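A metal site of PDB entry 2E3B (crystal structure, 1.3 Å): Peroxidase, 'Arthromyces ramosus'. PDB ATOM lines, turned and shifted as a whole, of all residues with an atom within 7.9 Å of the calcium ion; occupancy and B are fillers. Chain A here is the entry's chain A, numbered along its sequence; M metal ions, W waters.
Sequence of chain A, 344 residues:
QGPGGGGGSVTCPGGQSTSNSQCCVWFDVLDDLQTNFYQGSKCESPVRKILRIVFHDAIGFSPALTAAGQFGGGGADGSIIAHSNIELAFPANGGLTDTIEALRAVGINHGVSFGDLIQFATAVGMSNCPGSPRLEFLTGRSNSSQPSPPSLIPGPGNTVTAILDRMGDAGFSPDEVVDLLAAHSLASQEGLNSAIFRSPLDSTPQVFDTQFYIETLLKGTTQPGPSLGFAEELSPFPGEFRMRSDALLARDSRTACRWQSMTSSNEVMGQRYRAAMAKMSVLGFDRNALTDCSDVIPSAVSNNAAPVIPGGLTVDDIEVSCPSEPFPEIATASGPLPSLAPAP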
ATOM      1  N   ILE A  53      11.031   8.514 -18.334  1.00  0.00           N
ATOM      2  CA  ILE A  53      12.272   7.826 -18.533  1.00  0.00           C
ATOM      3  C   ILE A  53      13.438   8.462 -17.824  1.00  0.00           C
ATOM      4  O   ILE A  53      14.273   7.756 -17.278  1.00  0.00           O
ATOM      5  CB  ILE A  53      12.531   7.702 -20.056  1.00  0.00           C
ATOM      6  CG1 ILE A  53      11.501   6.732 -20.660  1.00  0.00           C
ATOM      7  CG2 ILE A  53      13.951   7.310 -20.340  1.00  0.00           C
ATOM      8  CD1 ILE A  53      11.414   6.811 -22.149  1.00  0.00           C
ATOM      9  N   VAL A  54      13.498   9.782 -17.744  1.00  0.00           N
ATOM     10  CA  VAL A  54      14.665  10.375 -17.104  1.00  0.00           C
ATOM     11  C   VAL A  54      14.657  10.069 -15.637  1.00  0.00           C
ATOM     12  O   VAL A  54      15.632   9.774 -15.016  1.00  0.00           O
ATOM     13  CB  VAL A  54      14.778  11.874 -17.440  1.00  0.00           C
ATOM     14  CG1 VAL A  54      13.678  12.678 -16.762  1.00  0.00           C
ATOM     15  CG2 VAL A  54      16.144  12.416 -17.048  1.00  0.00           C
ATOM     16  N   PHE A  55      13.467  10.148 -15.044  1.00  0.00           N
ATOM     17  CA  PHE A  55      13.313   9.812 -13.653  1.00  0.00           C
ATOM     18  C   PHE A  55      13.604   8.347 -13.421  1.00  0.00           C
ATOM     19  O   PHE A  55      14.345   7.986 -12.503  1.00  0.00           O
ATOM     20  CB  PHE A  55      11.892  10.184 -13.242  1.00  0.00           C
ATOM     21  CG  PHE A  55      11.493   9.821 -11.838  1.00  0.00           C
ATOM     22  CD1 PHE A  55      12.386   9.913 -10.771  1.00  0.00           C
ATOM     23  CD2 PHE A  55      10.218   9.365 -11.569  1.00  0.00           C
ATOM     24  CE1 PHE A  55      11.995   9.557  -9.518  1.00  0.00           C
ATOM     25  CE2 PHE A  55       9.820   8.997 -10.295  1.00  0.00           C
ATOM     26  CZ  PHE A  55      10.718   9.116  -9.241  1.00  0.00           C
ATOM     27  N   HIS A  56      13.010   7.505 -14.252  1.00  0.00           N
ATOM     28  CA  HIS A  56      13.214   6.088 -14.024  1.00  0.00           C
ATOM     29  C   HIS A  56      14.596   5.606 -14.375  1.00  0.00           C
ATOM     30  O   HIS A  56      15.023   4.557 -13.864  1.00  0.00           O
ATOM     31  CB  HIS A  56      12.134   5.281 -14.731  1.00  0.00           C
ATOM     32  CG  HIS A  56      10.770   5.565 -14.271  1.00  0.00           C
ATOM     33  ND1 HIS A  56       9.648   4.892 -14.703  1.00  0.00           N
ATOM     34  CD2 HIS A  56      10.360   6.485 -13.333  1.00  0.00           C
ATOM     35  CE1 HIS A  56       8.603   5.408 -14.072  1.00  0.00           C
ATOM     36  NE2 HIS A  56       9.004   6.357 -13.280  1.00  0.00           N
ATOM     37  N   ASP A  57      15.322   6.344 -15.196  1.00  0.00           N
ATOM     38  CA  ASP A  57      16.712   6.020 -15.393  1.00  0.00           C
ATOM     39  C   ASP A  57      17.497   6.425 -14.151  1.00  0.00           C
ATOM     40  O   ASP A  57      18.227   5.643 -13.568  1.00  0.00           O
ATOM     41  CB  ASP A  57      17.280   6.716 -16.638  1.00  0.00           C
ATOM     42  CG  ASP A  57      18.698   6.243 -16.881  1.00  0.00           C
ATOM     43  OD1 ASP A  57      18.965   5.078 -16.539  1.00  0.00           O
ATOM     44  OD2 ASP A  57      19.499   7.019 -17.421  1.00  0.00           O
ATOM     45  N   ALA A  58      17.313   7.659 -13.726  1.00  0.00           N
ATOM     46  CA  ALA A  58      18.145   8.213 -12.672  1.00  0.00           C
ATOM     47  C   ALA A  58      17.910   7.592 -11.302  1.00  0.00           C
ATOM     48  O   ALA A  58      18.852   7.448 -10.537  1.00  0.00           O
ATOM     49  CB  ALA A  58      17.986   9.727 -12.576  1.00  0.00           C
ATOM     50  N   ILE A  59      16.645   7.281 -11.030  1.00  0.00           N
ATOM     51  CA  ILE A  59      16.295   6.870  -9.684  1.00  0.00           C
ATOM     52  C   ILE A  59      16.749   5.445  -9.400  1.00  0.00           C
ATOM     53  O   ILE A  59      16.646   5.071  -8.240  1.00  0.00           O
ATOM     54  CB  ILE A  59      14.783   7.092  -9.468  1.00  0.00           C
ATOM     55  CG1 ILE A  59      14.483   7.394  -7.985  1.00  0.00           C
ATOM     56  CG2 ILE A  59      13.945   5.949 -10.032  1.00  0.00           C
ATOM     57  CD1 ILE A  59      15.171   8.661  -7.479  1.00  0.00           C
ATOM     58  N   GLY A  60      17.264   4.739 -10.389  1.00  0.00           N
ATOM     59  CA  GLY A  60      17.862   3.426 -10.165  1.00  0.00           C
ATOM     60  C   GLY A  60      19.268   3.680  -9.608  1.00  0.00           C
ATOM     61  O   GLY A  60      20.302   3.469 -10.211  1.00  0.00           O
ATOM     62  N   PHE A  61      19.235   4.111  -8.344  1.00  0.00           N
ATOM     63  CA  PHE A  61      20.436   4.538  -7.639  1.00  0.00           C
ATOM     64  C   PHE A  61      20.097   4.401  -6.182  1.00  0.00           C
ATOM     65  O   PHE A  61      19.124   4.991  -5.748  1.00  0.00           O
ATOM     66  CB  PHE A  61      20.752   5.974  -7.982  1.00  0.00           C
ATOM     67  CG  PHE A  61      22.043   6.444  -7.318  1.00  0.00           C
ATOM     68  CD1 PHE A  61      23.258   5.991  -7.791  1.00  0.00           C
ATOM     69  CD2 PHE A  61      21.985   7.302  -6.253  1.00  0.00           C
ATOM     70  CE1 PHE A  61      24.420   6.376  -7.170  1.00  0.00           C
ATOM     71  CE2 PHE A  61      23.153   7.722  -5.647  1.00  0.00           C
ATOM     72  CZ  PHE A  61      24.376   7.291  -6.120  1.00  0.00           C
ATOM     73  N   GLY A  73      22.756   0.351  -8.366  1.00  0.00           N
ATOM     74  CA  GLY A  73      22.365   1.084  -9.550  1.00  0.00           C
ATOM     75  C   GLY A  73      23.293   2.245  -9.856  1.00  0.00           C
ATOM     76  O   GLY A  73      23.867   2.855  -9.003  1.00  0.00           O
ATOM     77  N   GLY A  74      23.408   2.514 -11.141  1.00  0.00           N
ATOM     78  CA  GLY A  74      24.299   3.533 -11.603  1.00  0.00           C
ATOM     79  C   GLY A  74      23.675   4.861 -11.902  1.00  0.00           C
ATOM     80  O   GLY A  74      24.329   5.740 -12.447  1.00  0.00           O
ATOM     81  N   GLY A  75      22.427   5.039 -11.480  1.00  0.00           N
ATOM     82  CA  GLY A  75      21.808   6.350 -11.644  1.00  0.00           C
ATOM     83  C   GLY A  75      21.516   6.663 -13.092  1.00  0.00           C
ATOM     84  O   GLY A  75      20.933   5.865 -13.825  1.00  0.00           O
ATOM     85  N   ALA A  76      21.866   7.862 -13.500  1.00  0.00           N
ATOM     86  CA  ALA A  76      21.542   8.441 -14.797  1.00  0.00           C
ATOM     87  C   ALA A  76      22.425   7.854 -15.889  1.00  0.00           C
ATOM     88  O   ALA A  76      23.045   8.590 -16.662  1.00  0.00           O
ATOM     89  CB  ALA A  76      21.683   9.941 -14.683  1.00  0.00           C
ATOM     90  N   ASP A  77      22.502   6.549 -15.930  1.00  0.00           N
ATOM     91  CA  ASP A  77      23.495   5.809 -16.704  1.00  0.00           C
ATOM     92  C   ASP A  77      22.909   5.249 -17.988  1.00  0.00           C
ATOM     93  O   ASP A  77      23.609   4.514 -18.674  1.00  0.00           O
ATOM     94  CB  ASP A  77      24.022   4.659 -15.889  1.00  0.00           C
ATOM     95  CG  ASP A  77      22.987   3.733 -15.309  1.00  0.00           C
ATOM     96  OD1 ASP A  77      21.786   3.868 -15.616  1.00  0.00           O
ATOM     97  OD2 ASP A  77      23.419   2.810 -14.570  1.00  0.00           O
ATOM     98  N   GLY A  78      21.684   5.565 -18.323  1.00  0.00           N
ATOM     99  CA  GLY A  78      21.072   5.033 -19.530  1.00  0.00           C
ATOM    100  C   GLY A  78      20.698   3.572 -19.411  1.00  0.00           C
ATOM    101  O   GLY A  78      20.370   2.951 -20.407  1.00  0.00           O
ATOM    102  N   SER A  79      20.740   2.981 -18.228  1.00  0.00           N
ATOM    103  CA  SER A  79      20.509   1.581 -18.042  1.00  0.00           C
ATOM    104  C   SER A  79      19.091   1.201 -18.487  1.00  0.00           C
ATOM    105  O   SER A  79      18.884   0.092 -18.945  1.00  0.00           O
ATOM    106  CB  SER A  79      20.700   1.176 -16.589  1.00  0.00           C
ATOM    107  OG  SER A  79      19.738   1.837 -15.780  1.00  0.00           O
ATOM    108  N   ILE A  80      18.166   2.134 -18.383  1.00  0.00           N
ATOM    109  CA  ILE A  80      16.805   1.838 -18.794  1.00  0.00           C
ATOM    110  C   ILE A  80      16.727   1.570 -20.307  1.00  0.00           C
ATOM    111  O   ILE A  80      15.791   0.898 -20.734  1.00  0.00           O
ATOM    112  CB  ILE A  80      15.870   2.974 -18.349  1.00  0.00           C
ATOM    113  CG1 ILE A  80      14.426   2.554 -18.407  1.00  0.00           C
ATOM    114  CG2 ILE A  80      16.135   4.274 -19.105  1.00  0.00           C
ATOM    115  CD1 ILE A  80      13.467   3.545 -17.778  1.00  0.00           C
ATOM    116  N   ILE A  81      17.671   2.110 -21.058  1.00  0.00           N
ATOM    117  CA  ILE A  81      17.785   1.769 -22.483  1.00  0.00           C
ATOM    118  C   ILE A  81      18.681   0.570 -22.692  1.00  0.00           C
ATOM    119  O   ILE A  81      18.272  -0.434 -23.291  1.00  0.00           O
ATOM    120  CB  ILE A  81      18.284   2.947 -23.313  1.00  0.00           C
ATOM    121  CG1 ILE A  81      17.380   4.163 -23.166  1.00  0.00           C
ATOM    122  CG2 ILE A  81      18.435   2.543 -24.784  1.00  0.00           C
ATOM    123  CD1 ILE A  81      17.907   5.430 -23.815  1.00  0.00           C
ATOM    124  N   HIS A  83      19.643  -1.807 -20.803  1.00  0.00           N
ATOM    125  CA  HIS A  83      19.083  -2.946 -20.157  1.00  0.00           C
ATOM    126  C   HIS A  83      17.566  -2.847 -20.061  1.00  0.00           C
ATOM    127  O   HIS A  83      16.929  -3.218 -19.109  1.00  0.00           O
ATOM    128  CB  HIS A  83      19.682  -3.075 -18.742  1.00  0.00           C
ATOM    129  CG  HIS A  83      21.157  -3.193 -18.867  1.00  0.00           C
ATOM    130  ND1 HIS A  83      21.793  -4.277 -19.417  1.00  0.00           N
ATOM    131  CD2 HIS A  83      22.157  -2.315 -18.525  1.00  0.00           C
ATOM    132  CE1 HIS A  83      23.099  -4.101 -19.387  1.00  0.00           C
ATOM    133  NE2 HIS A  83      23.360  -2.917 -18.866  1.00  0.00           N
ATOM    134  N   GLU A  87      14.725  -3.685 -17.318  1.00  0.00           N
ATOM    135  CA  GLU A  87      14.069  -2.589 -16.606  1.00  0.00           C
ATOM    136  C   GLU A  87      12.656  -2.353 -17.072  1.00  0.00           C
ATOM    137  O   GLU A  87      11.870  -1.908 -16.223  1.00  0.00           O
ATOM    138  CB  GLU A  87      14.900  -1.296 -16.714  1.00  0.00           C
ATOM    139  CG  GLU A  87      16.275  -1.475 -16.117  1.00  0.00           C
ATOM    140  CD  GLU A  87      16.997  -0.187 -15.768  1.00  0.00           C
ATOM    141  OE1 GLU A  87      16.332   0.863 -15.669  1.00  0.00           O
ATOM    142  OE2 GLU A  87      18.238  -0.250 -15.652  1.00  0.00           O
ATOM    143  N   GLY A 115      22.885   7.489 -21.328  1.00  0.00           N
ATOM    144  CA  GLY A 115      22.522   8.313 -20.165  1.00  0.00           C
ATOM    145  C   GLY A 115      22.548   9.768 -20.534  1.00  0.00           C
ATOM    146  O   GLY A 115      21.699  10.537 -20.101  1.00  0.00           O
ATOM    147  N   ILE A 118      19.334  10.565 -22.660  1.00  0.00           N
ATOM    148  CA  ILE A 118      18.089  10.750 -21.907  1.00  0.00           C
ATOM    149  C   ILE A 118      18.045  12.121 -21.297  1.00  0.00           C
ATOM    150  O   ILE A 118      17.044  12.825 -21.332  1.00  0.00           O
ATOM    151  CB  ILE A 118      17.940   9.643 -20.854  1.00  0.00           C
ATOM    152  CG1 ILE A 118      17.705   8.311 -21.563  1.00  0.00           C
ATOM    153  CG2 ILE A 118      16.841   9.963 -19.846  1.00  0.00           C
ATOM    154  CD1 ILE A 118      17.790   7.122 -20.645  1.00  0.00           C
ATOM    155  N   SER A 145      26.608   0.649 -18.502  1.00  0.00           N
ATOM    156  CA  SER A 145      25.692   0.516 -17.361  1.00  0.00           C
ATOM    157  C   SER A 145      25.467  -0.950 -17.047  1.00  0.00           C
ATOM    158  O   SER A 145      25.606  -1.835 -17.896  1.00  0.00           O
ATOM    159  CB  SER A 145      24.382   1.219 -17.644  1.00  0.00           C
ATOM    160  OG  SER A 145      23.680   0.576 -18.690  1.00  0.00           O
ATOM    161  N   GLN A 146      25.045  -1.203 -15.825  1.00  0.00           N
ATOM    162  CA  GLN A 146      24.508  -2.451 -15.357  1.00  0.00           C
ATOM    163  C   GLN A 146      23.013  -2.221 -15.188  1.00  0.00           C
ATOM    164  O   GLN A 146      22.583  -1.050 -15.047  1.00  0.00           O
ATOM    165  CB  GLN A 146      25.089  -2.912 -14.016  1.00  0.00           C
ATOM    166  CG  GLN A 146      26.504  -3.461 -14.061  1.00  0.00           C
ATOM    167  CD  GLN A 146      27.220  -3.256 -12.723  1.00  0.00           C
ATOM    168  OE1 GLN A 146      28.065  -2.357 -12.662  1.00  0.00           O
ATOM    169  NE2 GLN A 146      26.869  -4.023 -11.691  1.00  0.00           N
ATOM    170  N   PRO A 147      22.207  -3.274 -15.180  1.00  0.00           N
ATOM    171  CA  PRO A 147      20.781  -3.061 -14.996  1.00  0.00           C
ATOM    172  C   PRO A 147      20.512  -2.460 -13.626  1.00  0.00           C
ATOM    173  O   PRO A 147      21.102  -2.831 -12.621  1.00  0.00           O
ATOM    174  CB  PRO A 147      20.192  -4.473 -15.026  1.00  0.00           C
ATOM    175  CG  PRO A 147      21.225  -5.271 -15.789  1.00  0.00           C
ATOM    176  CD  PRO A 147      22.533  -4.702 -15.339  1.00  0.00           C
ATOM    177  N   SER A 148      19.580  -1.509 -13.583  1.00  0.00           N
ATOM    178  CA  SER A 148      19.083  -1.084 -12.300  1.00  0.00           C
ATOM    179  C   SER A 148      18.598  -2.263 -11.466  1.00  0.00           C
ATOM    180  O   SER A 148      17.925  -3.130 -11.993  1.00  0.00           O
ATOM    181  CB  SER A 148      17.864  -0.144 -12.467  1.00  0.00           C
ATOM    182  OG  SER A 148      17.368   0.281 -11.207  1.00  0.00           O
ATOM    183  N   PRO A 149      18.857  -2.234 -10.183  1.00  0.00           N
ATOM    184  CA  PRO A 149      18.138  -3.129  -9.286  1.00  0.00           C
ATOM    185  C   PRO A 149      16.647  -2.860  -9.444  1.00  0.00           C
ATOM    186  O   PRO A 149      16.224  -1.747  -9.813  1.00  0.00           O
ATOM    187  CB  PRO A 149      18.556  -2.677  -7.894  1.00  0.00           C
ATOM    188  CG  PRO A 149      19.960  -2.178  -8.142  1.00  0.00           C
ATOM    189  CD  PRO A 149      19.832  -1.421  -9.432  1.00  0.00           C
ATOM    190  N   LEU A 283      22.942  11.677 -10.648  1.00  0.00           N
ATOM    191  CA  LEU A 283      23.036  10.532  -9.751  1.00  0.00           C
ATOM    192  C   LEU A 283      23.877   9.472 -10.434  1.00  0.00           C
ATOM    193  O   LEU A 283      23.580   9.117 -11.567  1.00  0.00           O
ATOM    194  CB  LEU A 283      21.645   9.971  -9.416  1.00  0.00           C
ATOM    195  CG  LEU A 283      20.732  10.929  -8.621  1.00  0.00           C
ATOM    196  CD1 LEU A 283      19.409  10.257  -8.380  1.00  0.00           C
ATOM    197  CD2 LEU A 283      21.311  11.325  -7.287  1.00  0.00           C
ATOM    198  N   PHE A 285      27.172   9.959 -10.920  1.00  0.00           N
ATOM    199  CA  PHE A 285      28.212  10.679 -11.632  1.00  0.00           C
ATOM    200  C   PHE A 285      28.708  11.878 -10.839  1.00  0.00           C
ATOM    201  O   PHE A 285      28.032  12.421  -9.978  1.00  0.00           O
ATOM    202  CB  PHE A 285      27.705  11.231 -12.987  1.00  0.00           C
ATOM    203  CG  PHE A 285      27.262  10.074 -13.860  1.00  0.00           C
ATOM    204  CD1 PHE A 285      25.949   9.638 -13.781  1.00  0.00           C
ATOM    205  CD2 PHE A 285      28.153   9.430 -14.660  1.00  0.00           C
ATOM    206  CE1 PHE A 285      25.573   8.526 -14.504  1.00  0.00           C
ATOM    207  CE2 PHE A 285      27.790   8.357 -15.416  1.00  0.00           C
ATOM    208  CZ  PHE A 285      26.474   7.903 -15.329  1.00  0.00           C
HETATM  209 CA    CA M   1      19.667   3.966 -14.624  1.00  0.00          CA
HETATM  210  O   HOH W   1      17.446   2.960 -14.450  1.00  0.00           O
HETATM  211  O   HOH W   2      20.118   2.658 -12.752  1.00  0.00           O
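Water W1 bridges OE1 of Glu 87 and O of His 56.
The calcium ion is bound by the side-chain carboxylate (OD1) of Asp 57 (2.3 Å), water W2 (2.3 Å), the side-chain carboxylate (OD1) of Asp 77 (2.3 Å), the backbone carbonyl oxygen (O) of Gly 75 (2.4 Å), the side-chain hydroxyl (OG) of Ser 79 (2.4 Å), water W1 (2.4 Å) and the backbone carbonyl oxygen (O) of Asp 57 (2.4 Å).
The calcium ion has seven donor atoms within binding distance.
The backbone NH (N) of Gly 78 sits at hydrogen-bond distance from the side-chain carboxylate (OD2) of Asp 57 (2.8 Å).
The side-chain carboxylate (OD2) of Asp 77 sits close to the backbone NH (N) of Gly 74 (3.4 Å).
O of Gly 60 sits at hydrogen-bond distance from N of Gly 75 (2.9 Å).
The side-chain hydroxyl (OG) of Ser 79 lies close to the side-chain carboxylate (OE2) of Glu 87 (2.6 Å).
Of the 29 residues printed, 4 come within 4 Å of the calcium ion.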
